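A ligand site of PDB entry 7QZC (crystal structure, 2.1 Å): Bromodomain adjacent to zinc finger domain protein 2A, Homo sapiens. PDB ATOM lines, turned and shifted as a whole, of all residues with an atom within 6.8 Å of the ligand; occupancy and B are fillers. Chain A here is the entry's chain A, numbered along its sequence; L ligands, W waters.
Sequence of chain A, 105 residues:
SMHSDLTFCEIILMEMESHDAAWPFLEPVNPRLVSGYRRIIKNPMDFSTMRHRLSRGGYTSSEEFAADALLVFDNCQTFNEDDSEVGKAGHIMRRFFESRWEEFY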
ATOM      1  N   TRP A  23     -30.540 -26.770 -28.274  1.00  0.00           N
ATOM      2  CA  TRP A  23     -30.060 -26.321 -26.968  1.00  0.00           C
ATOM      3  C   TRP A  23     -28.582 -25.950 -26.923  1.00  0.00           C
ATOM      4  O   TRP A  23     -28.249 -25.045 -26.146  1.00  0.00           O
ATOM      5  CB  TRP A  23     -30.395 -27.394 -25.920  1.00  0.00           C
ATOM      6  CG  TRP A  23     -29.738 -28.729 -26.145  1.00  0.00           C
ATOM      7  CD1 TRP A  23     -30.257 -29.786 -26.826  1.00  0.00           C
ATOM      8  CD2 TRP A  23     -28.445 -29.132 -25.684  1.00  0.00           C
ATOM      9  NE1 TRP A  23     -29.356 -30.825 -26.831  1.00  0.00           N
ATOM     10  CE2 TRP A  23     -28.235 -30.459 -26.139  1.00  0.00           C
ATOM     11  CE3 TRP A  23     -27.436 -28.504 -24.959  1.00  0.00           C
ATOM     12  CZ2 TRP A  23     -27.069 -31.157 -25.865  1.00  0.00           C
ATOM     13  CZ3 TRP A  23     -26.270 -29.202 -24.685  1.00  0.00           C
ATOM     14  CH2 TRP A  23     -26.094 -30.519 -25.138  1.00  0.00           C
ATOM     15  N   PRO A  24     -27.652 -26.539 -27.697  1.00  0.00           N
ATOM     16  CA  PRO A  24     -26.263 -26.060 -27.625  1.00  0.00           C
ATOM     17  C   PRO A  24     -26.052 -24.712 -28.273  1.00  0.00           C
ATOM     18  O   PRO A  24     -25.045 -24.054 -27.961  1.00  0.00           O
ATOM     19  CB  PRO A  24     -25.448 -27.143 -28.348  1.00  0.00           C
ATOM     20  CG  PRO A  24     -26.397 -28.321 -28.476  1.00  0.00           C
ATOM     21  CD  PRO A  24     -27.729 -27.688 -28.605  1.00  0.00           C
ATOM     22  N   PHE A  25     -26.953 -24.266 -29.145  1.00  0.00           N
ATOM     23  CA  PHE A  25     -26.679 -23.145 -30.029  1.00  0.00           C
ATOM     24  C   PHE A  25     -27.545 -21.919 -29.766  1.00  0.00           C
ATOM     25  O   PHE A  25     -27.485 -20.947 -30.523  1.00  0.00           O
ATOM     26  CB  PHE A  25     -26.839 -23.599 -31.478  1.00  0.00           C
ATOM     27  CG  PHE A  25     -26.240 -24.944 -31.735  1.00  0.00           C
ATOM     28  CD1 PHE A  25     -24.883 -25.105 -31.883  1.00  0.00           C
ATOM     29  CD2 PHE A  25     -27.045 -26.067 -31.805  1.00  0.00           C
ATOM     30  CE1 PHE A  25     -24.328 -26.337 -32.101  1.00  0.00           C
ATOM     31  CE2 PHE A  25     -26.494 -27.313 -32.022  1.00  0.00           C
ATOM     32  CZ  PHE A  25     -25.127 -27.438 -32.161  1.00  0.00           C
ATOM     33  N   LEU A  26     -28.330 -21.932 -28.678  1.00  0.00           N
ATOM     34  CA  LEU A  26     -29.203 -20.804 -28.382  1.00  0.00           C
ATOM     35  C   LEU A  26     -28.436 -19.575 -27.887  1.00  0.00           C
ATOM     36  O   LEU A  26     -28.899 -18.449 -28.098  1.00  0.00           O
ATOM     37  CB  LEU A  26     -30.258 -21.220 -27.346  1.00  0.00           C
ATOM     38  CG  LEU A  26     -31.175 -22.347 -27.814  1.00  0.00           C
ATOM     39  CD1 LEU A  26     -32.286 -22.634 -26.809  1.00  0.00           C
ATOM     40  CD2 LEU A  26     -31.774 -21.997 -29.174  1.00  0.00           C
ATOM     41  N   GLU A  27     -27.293 -19.749 -27.240  1.00  0.00           N
ATOM     42  CA  GLU A  27     -26.496 -18.657 -26.703  1.00  0.00           C
ATOM     43  C   GLU A  27     -25.041 -18.827 -27.112  1.00  0.00           C
ATOM     44  O   GLU A  27     -24.602 -19.945 -27.380  1.00  0.00           O
ATOM     45  CB  GLU A  27     -26.576 -18.614 -25.168  1.00  0.00           C
ATOM     46  CG  GLU A  27     -27.961 -18.333 -24.580  1.00  0.00           C
ATOM     47  CD  GLU A  27     -28.572 -17.025 -25.046  1.00  0.00           C
ATOM     48  OE1 GLU A  27     -29.762 -17.041 -25.456  1.00  0.00           O
ATOM     49  OE2 GLU A  27     -27.898 -15.979 -24.997  1.00  0.00           O
ATOM     50  N   PRO A  28     -24.259 -17.724 -27.145  1.00  0.00           N
ATOM     51  CA  PRO A  28     -22.809 -17.854 -27.389  1.00  0.00           C
ATOM     52  C   PRO A  28     -22.169 -18.831 -26.423  1.00  0.00           C
ATOM     53  O   PRO A  28     -22.560 -18.927 -25.259  1.00  0.00           O
ATOM     54  CB  PRO A  28     -22.278 -16.427 -27.155  1.00  0.00           C
ATOM     55  CG  PRO A  28     -23.454 -15.547 -27.341  1.00  0.00           C
ATOM     56  CD  PRO A  28     -24.654 -16.327 -26.912  1.00  0.00           C
ATOM     57  N   VAL A  29     -21.181 -19.568 -26.909  1.00  0.00           N
ATOM     58  CA  VAL A  29     -20.346 -20.347 -26.011  1.00  0.00           C
ATOM     59  C   VAL A  29     -19.572 -19.408 -25.101  1.00  0.00           C
ATOM     60  O   VAL A  29     -19.044 -18.384 -25.561  1.00  0.00           O
ATOM     61  CB  VAL A  29     -19.397 -21.253 -26.808  1.00  0.00           C
ATOM     62  CG1 VAL A  29     -18.399 -21.903 -25.872  1.00  0.00           C
ATOM     63  CG2 VAL A  29     -20.212 -22.300 -27.582  1.00  0.00           C
ATOM     64  N   ASN A  30     -19.533 -19.732 -23.816  1.00  0.00           N
ATOM     65  CA  ASN A  30     -18.755 -18.966 -22.859  1.00  0.00           C
ATOM     66  C   ASN A  30     -17.339 -19.518 -22.797  1.00  0.00           C
ATOM     67  O   ASN A  30     -17.107 -20.577 -22.192  1.00  0.00           O
ATOM     68  CB  ASN A  30     -19.421 -18.995 -21.483  1.00  0.00           C
ATOM     69  CG  ASN A  30     -18.826 -17.996 -20.528  1.00  0.00           C
ATOM     70  OD1 ASN A  30     -17.669 -17.601 -20.666  1.00  0.00           O
ATOM     71  ND2 ASN A  30     -19.606 -17.579 -19.550  1.00  0.00           N
ATOM     72  N   PRO A  31     -16.362 -18.837 -23.402  1.00  0.00           N
ATOM     73  CA  PRO A  31     -14.973 -19.349 -23.379  1.00  0.00           C
ATOM     74  C   PRO A  31     -14.425 -19.548 -21.970  1.00  0.00           C
ATOM     75  O   PRO A  31     -13.534 -20.379 -21.775  1.00  0.00           O
ATOM     76  CB  PRO A  31     -14.185 -18.280 -24.149  1.00  0.00           C
ATOM     77  CG  PRO A  31     -14.997 -17.018 -23.959  1.00  0.00           C
ATOM     78  CD  PRO A  31     -16.435 -17.487 -23.991  1.00  0.00           C
ATOM     79  N   LEU A  33     -15.898 -21.007 -19.667  1.00  0.00           N
ATOM     80  CA  LEU A  33     -16.364 -22.307 -19.218  1.00  0.00           C
ATOM     81  C   LEU A  33     -15.862 -23.453 -20.085  1.00  0.00           C
ATOM     82  O   LEU A  33     -15.978 -24.607 -19.670  1.00  0.00           O
ATOM     83  CB  LEU A  33     -17.900 -22.316 -19.191  1.00  0.00           C
ATOM     84  CG  LEU A  33     -18.546 -21.176 -18.407  1.00  0.00           C
ATOM     85  CD1 LEU A  33     -20.070 -21.261 -18.436  1.00  0.00           C
ATOM     86  CD2 LEU A  33     -18.038 -21.155 -16.973  1.00  0.00           C
ATOM     87  N   VAL A  34     -15.294 -23.169 -21.253  1.00  0.00           N
ATOM     88  CA  VAL A  34     -14.908 -24.198 -22.207  1.00  0.00           C
ATOM     89  C   VAL A  34     -13.437 -24.001 -22.512  1.00  0.00           C
ATOM     90  O   VAL A  34     -13.069 -23.140 -23.319  1.00  0.00           O
ATOM     91  CB  VAL A  34     -15.749 -24.149 -23.486  1.00  0.00           C
ATOM     92  CG1 VAL A  34     -15.312 -25.256 -24.424  1.00  0.00           C
ATOM     93  CG2 VAL A  34     -17.227 -24.273 -23.133  1.00  0.00           C
ATOM     94  N   TYR A  37     -11.606 -23.168 -26.211  1.00  0.00           N
ATOM     95  CA  TYR A  37     -12.553 -22.749 -27.246  1.00  0.00           C
ATOM     96  C   TYR A  37     -12.057 -21.507 -27.960  1.00  0.00           C
ATOM     97  O   TYR A  37     -12.053 -21.431 -29.191  1.00  0.00           O
ATOM     98  CB  TYR A  37     -13.941 -22.509 -26.638  1.00  0.00           C
ATOM     99  CG  TYR A  37     -15.022 -22.440 -27.708  1.00  0.00           C
ATOM    100  CD1 TYR A  37     -15.572 -23.591 -28.239  1.00  0.00           C
ATOM    101  CD2 TYR A  37     -15.457 -21.224 -28.188  1.00  0.00           C
ATOM    102  CE1 TYR A  37     -16.549 -23.533 -29.221  1.00  0.00           C
ATOM    103  CE2 TYR A  37     -16.420 -21.134 -29.170  1.00  0.00           C
ATOM    104  CZ  TYR A  37     -16.966 -22.299 -29.683  1.00  0.00           C
ATOM    105  OH  TYR A  37     -17.933 -22.206 -30.657  1.00  0.00           O
ATOM    106  N   ILE A  41     -11.649 -21.840 -31.985  1.00  0.00           N
ATOM    107  CA  ILE A  41     -12.769 -21.334 -32.776  1.00  0.00           C
ATOM    108  C   ILE A  41     -12.532 -19.857 -33.038  1.00  0.00           C
ATOM    109  O   ILE A  41     -12.703 -19.018 -32.146  1.00  0.00           O
ATOM    110  CB  ILE A  41     -14.105 -21.577 -32.070  1.00  0.00           C
ATOM    111  CG1 ILE A  41     -14.411 -23.060 -32.049  1.00  0.00           C
ATOM    112  CG2 ILE A  41     -15.229 -20.801 -32.757  1.00  0.00           C
ATOM    113  CD1 ILE A  41     -14.475 -23.675 -33.447  1.00  0.00           C
ATOM    114  N   MET A  45     -20.264 -18.264 -33.457  1.00  0.00           N
ATOM    115  CA  MET A  45     -21.571 -17.878 -33.981  1.00  0.00           C
ATOM    116  C   MET A  45     -22.622 -18.736 -33.291  1.00  0.00           C
ATOM    117  O   MET A  45     -22.380 -19.896 -32.985  1.00  0.00           O
ATOM    118  CB  MET A  45     -21.613 -18.041 -35.509  1.00  0.00           C
ATOM    119  CG  MET A  45     -22.896 -17.565 -36.162  1.00  0.00           C
ATOM    120  SD  MET A  45     -23.426 -15.927 -35.668  1.00  0.00           S
ATOM    121  CE  MET A  45     -21.969 -14.970 -36.123  1.00  0.00           C
ATOM    122  N   VAL A  72     -22.086 -21.855 -37.506  1.00  0.00           N
ATOM    123  CA  VAL A  72     -22.503 -22.536 -36.287  1.00  0.00           C
ATOM    124  C   VAL A  72     -22.133 -24.011 -36.347  1.00  0.00           C
ATOM    125  O   VAL A  72     -21.528 -24.563 -35.418  1.00  0.00           O
ATOM    126  CB  VAL A  72     -24.002 -22.347 -36.028  1.00  0.00           C
ATOM    127  CG1 VAL A  72     -24.403 -22.991 -34.715  1.00  0.00           C
ATOM    128  CG2 VAL A  72     -24.353 -20.876 -36.039  1.00  0.00           C
ATOM    129  N   ASN A  75     -18.225 -24.641 -36.728  1.00  0.00           N
ATOM    130  CA  ASN A  75     -17.588 -24.521 -35.410  1.00  0.00           C
ATOM    131  C   ASN A  75     -17.889 -25.734 -34.554  1.00  0.00           C
ATOM    132  O   ASN A  75     -17.005 -26.253 -33.863  1.00  0.00           O
ATOM    133  CB  ASN A  75     -18.065 -23.256 -34.692  1.00  0.00           C
ATOM    134  CG  ASN A  75     -17.599 -21.980 -35.361  1.00  0.00           C
ATOM    135  OD1 ASN A  75     -16.641 -21.988 -36.128  1.00  0.00           O
ATOM    136  ND2 ASN A  75     -18.308 -20.884 -35.091  1.00  0.00           N
ATOM    137  N   CYS A  76     -19.132 -26.213 -34.599  1.00  0.00           N
ATOM    138  CA  CYS A  76     -19.541 -27.333 -33.771  1.00  0.00           C
ATOM    139  C   CYS A  76     -18.719 -28.581 -34.078  1.00  0.00           C
ATOM    140  O   CYS A  76     -18.230 -29.265 -33.170  1.00  0.00           O
ATOM    141  CB  CYS A  76     -21.025 -27.609 -33.976  1.00  0.00           C
ATOM    142  SG  CYS A  76     -21.640 -28.972 -32.967  1.00  0.00           S
ATOM    143  N   PHE A  79     -14.937 -28.321 -32.959  1.00  0.00           N
ATOM    144  CA  PHE A  79     -14.569 -28.413 -31.553  1.00  0.00           C
ATOM    145  C   PHE A  79     -15.067 -29.678 -30.858  1.00  0.00           C
ATOM    146  O   PHE A  79     -14.414 -30.145 -29.911  1.00  0.00           O
ATOM    147  CB  PHE A  79     -15.093 -27.192 -30.803  1.00  0.00           C
ATOM    148  CG  PHE A  79     -14.452 -27.018 -29.461  1.00  0.00           C
ATOM    149  CD1 PHE A  79     -13.259 -26.342 -29.355  1.00  0.00           C
ATOM    150  CD2 PHE A  79     -15.026 -27.555 -28.337  1.00  0.00           C
ATOM    151  CE1 PHE A  79     -12.655 -26.193 -28.135  1.00  0.00           C
ATOM    152  CE2 PHE A  79     -14.427 -27.403 -27.109  1.00  0.00           C
ATOM    153  CZ  PHE A  79     -13.238 -26.720 -27.007  1.00  0.00           C
ATOM    154  N   ASN A  80     -16.192 -30.242 -31.275  1.00  0.00           N
ATOM    155  CA  ASN A  80     -16.834 -31.341 -30.555  1.00  0.00           C
ATOM    156  C   ASN A  80     -16.712 -32.646 -31.317  1.00  0.00           C
ATOM    157  O   ASN A  80     -16.802 -32.670 -32.553  1.00  0.00           O
ATOM    158  CB  ASN A  80     -18.311 -31.049 -30.310  1.00  0.00           C
ATOM    159  CG  ASN A  80     -18.534 -29.715 -29.674  1.00  0.00           C
ATOM    160  OD1 ASN A  80     -18.450 -29.581 -28.459  1.00  0.00           O
ATOM    161  ND2 ASN A  80     -18.832 -28.704 -30.484  1.00  0.00           N
ATOM    162  N   GLU A  85     -22.308 -35.223 -26.909  1.00  0.00           N
ATOM    163  CA  GLU A  85     -23.695 -34.798 -26.777  1.00  0.00           C
ATOM    164  C   GLU A  85     -23.971 -33.568 -27.620  1.00  0.00           C
ATOM    165  O   GLU A  85     -25.008 -33.461 -28.281  1.00  0.00           O
ATOM    166  CB  GLU A  85     -24.024 -34.556 -25.309  1.00  0.00           C
ATOM    167  CG  GLU A  85     -25.474 -34.796 -24.944  1.00  0.00           C
ATOM    168  CD  GLU A  85     -25.936 -36.214 -25.270  1.00  0.00           C
ATOM    169  OE1 GLU A  85     -25.116 -37.161 -25.241  1.00  0.00           O
ATOM    170  OE2 GLU A  85     -27.147 -36.374 -25.559  1.00  0.00           O
ATOM    171  N   VAL A  86     -23.028 -32.618 -27.648  1.00  0.00           N
ATOM    172  CA  VAL A  86     -23.185 -31.424 -28.460  1.00  0.00           C
ATOM    173  C   VAL A  86     -22.984 -31.736 -29.937  1.00  0.00           C
ATOM    174  O   VAL A  86     -23.720 -31.238 -30.798  1.00  0.00           O
ATOM    175  CB  VAL A  86     -22.215 -30.319 -27.990  1.00  0.00           C
ATOM    176  CG1 VAL A  86     -22.163 -29.196 -29.005  1.00  0.00           C
ATOM    177  CG2 VAL A  86     -22.619 -29.791 -26.595  1.00  0.00           C
HETATM  178  C1  LIG L   1     -20.083 -28.144 -24.647  1.00  0.00           C
HETATM  179  C2  LIG L   1     -20.356 -26.622 -24.590  1.00  0.00           C
HETATM  180  C3  LIG L   1     -21.160 -26.096 -25.855  1.00  0.00           C
HETATM  181  C4  LIG L   1     -22.542 -25.705 -25.901  1.00  0.00           C
HETATM  182  C5  LIG L   1     -23.424 -25.722 -24.822  1.00  0.00           C
HETATM  183  C6  LIG L   1     -24.340 -24.705 -24.640  1.00  0.00           C
HETATM  184  C7  LIG L   1     -24.329 -26.628 -22.938  1.00  0.00           C
HETATM  185  C8  LIG L   1     -25.090 -27.129 -20.553  1.00  0.00           C
HETATM  186  C9  LIG L   1     -25.559 -28.280 -19.681  1.00  0.00           C
HETATM  187  C10 LIG L   1     -23.966 -29.716 -20.639  1.00  0.00           C
HETATM  188  C11 LIG L   1     -23.450 -28.581 -21.538  1.00  0.00           C
HETATM  189  C12 LIG L   1     -22.304 -27.871 -20.815  1.00  0.00           C
HETATM  190  C13 LIG L   1     -21.323 -25.783 -19.718  1.00  0.00           C
HETATM  191  C14 LIG L   1     -20.369 -25.125 -20.746  1.00  0.00           C
HETATM  192  C15 LIG L   1     -21.004 -23.945 -21.442  1.00  0.00           C
HETATM  193  C16 LIG L   1     -22.340 -23.579 -21.395  1.00  0.00           C
HETATM  194  C17 LIG L   1     -22.475 -22.412 -22.186  1.00  0.00           C
HETATM  195  C18 LIG L   1     -21.727 -25.441 -27.954  1.00  0.00           C
HETATM  196  C19 LIG L   1     -21.660 -25.103 -29.467  1.00  0.00           C
HETATM  197  C20 LIG L   1     -20.649 -25.928 -27.157  1.00  0.00           C
HETATM  198  C21 LIG L   1     -19.205 -26.212 -27.625  1.00  0.00           C
HETATM  199  C22 LIG L   1     -18.128 -26.545 -26.620  1.00  0.00           C
HETATM  200  N1  LIG L   1     -24.522 -27.580 -21.849  1.00  0.00           N
HETATM  201  N2  LIG L   1     -24.530 -29.248 -19.452  1.00  0.00           N
HETATM  202  N3  LIG L   1     -22.443 -26.474 -20.408  1.00  0.00           N
HETATM  203  N4  LIG L   1     -21.288 -22.105 -22.664  1.00  0.00           N
HETATM  204  N5  LIG L   1     -23.434 -26.715 -23.924  1.00  0.00           N
HETATM  205  N6  LIG L   1     -22.840 -25.329 -27.151  1.00  0.00           N
HETATM  206  O1  LIG L   1     -21.275 -28.470 -20.576  1.00  0.00           O
HETATM  207  O2  LIG L   1     -20.366 -23.021 -22.226  1.00  0.00           O
HETATM  208  O3  LIG L   1     -18.933 -26.168 -28.821  1.00  0.00           O
HETATM  209  S1  LIG L   1     -25.209 -25.158 -23.188  1.00  0.00           S
HETATM  210  O   HOH W   1     -24.631 -21.260 -25.184  1.00  0.00           O
HETATM  211  O   HOH W   2     -21.249 -24.237 -32.653  1.00  0.00           O
HETATM  212  O   HOH W   3     -24.295 -32.533 -22.374  1.00  0.00           O
HETATM  213  O   HOH W   4     -18.869 -24.782 -31.301  1.00  0.00           O
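The backbone carbonyl oxygen (O) of Pro 24 is in hydrogen-bond range of a nitrogen (N6) of the ligand (2.7 Å).
The side-chain amide nitrogen (ND2) of Asn 80 is in hydrogen-bond range of an oxygen (O3) of the ligand, at 3.0 Å.
The backbone NH (N) of Asn 30 sits at hydrogen-bond distance from a nitrogen (N4) of the ligand (3.2 Å).
The side-chain amide nitrogen (ND2) of Asn 80 sits at hydrogen-bond distance from the backbone carbonyl oxygen (O) of Cys 76, 2.8 Å away.
The backbone carbonyl oxygen (O) of Val 86 sits at hydrogen-bond distance from the side-chain sulfur (SG) of Cys 76 (3.8 Å).
Residues that only touch the ligand: Trp 23, Phe 25, Val 29, Leu 33, Val 34, Tyr 37, Phe 79 and Val 86.
Within 4 Å of the ligand: Trp 23, Pro 24, Phe 25, Val 29, Asn 30, Leu 33, Val 34, Tyr 37, Phe 79, Asn 80 and Val 86.
Water W4 lies within hydrogen-bond range of OH of Tyr 37 (2.8 Å), O3 of the ligand (2.8 Å) and O of Asn 75 (3.5 Å).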
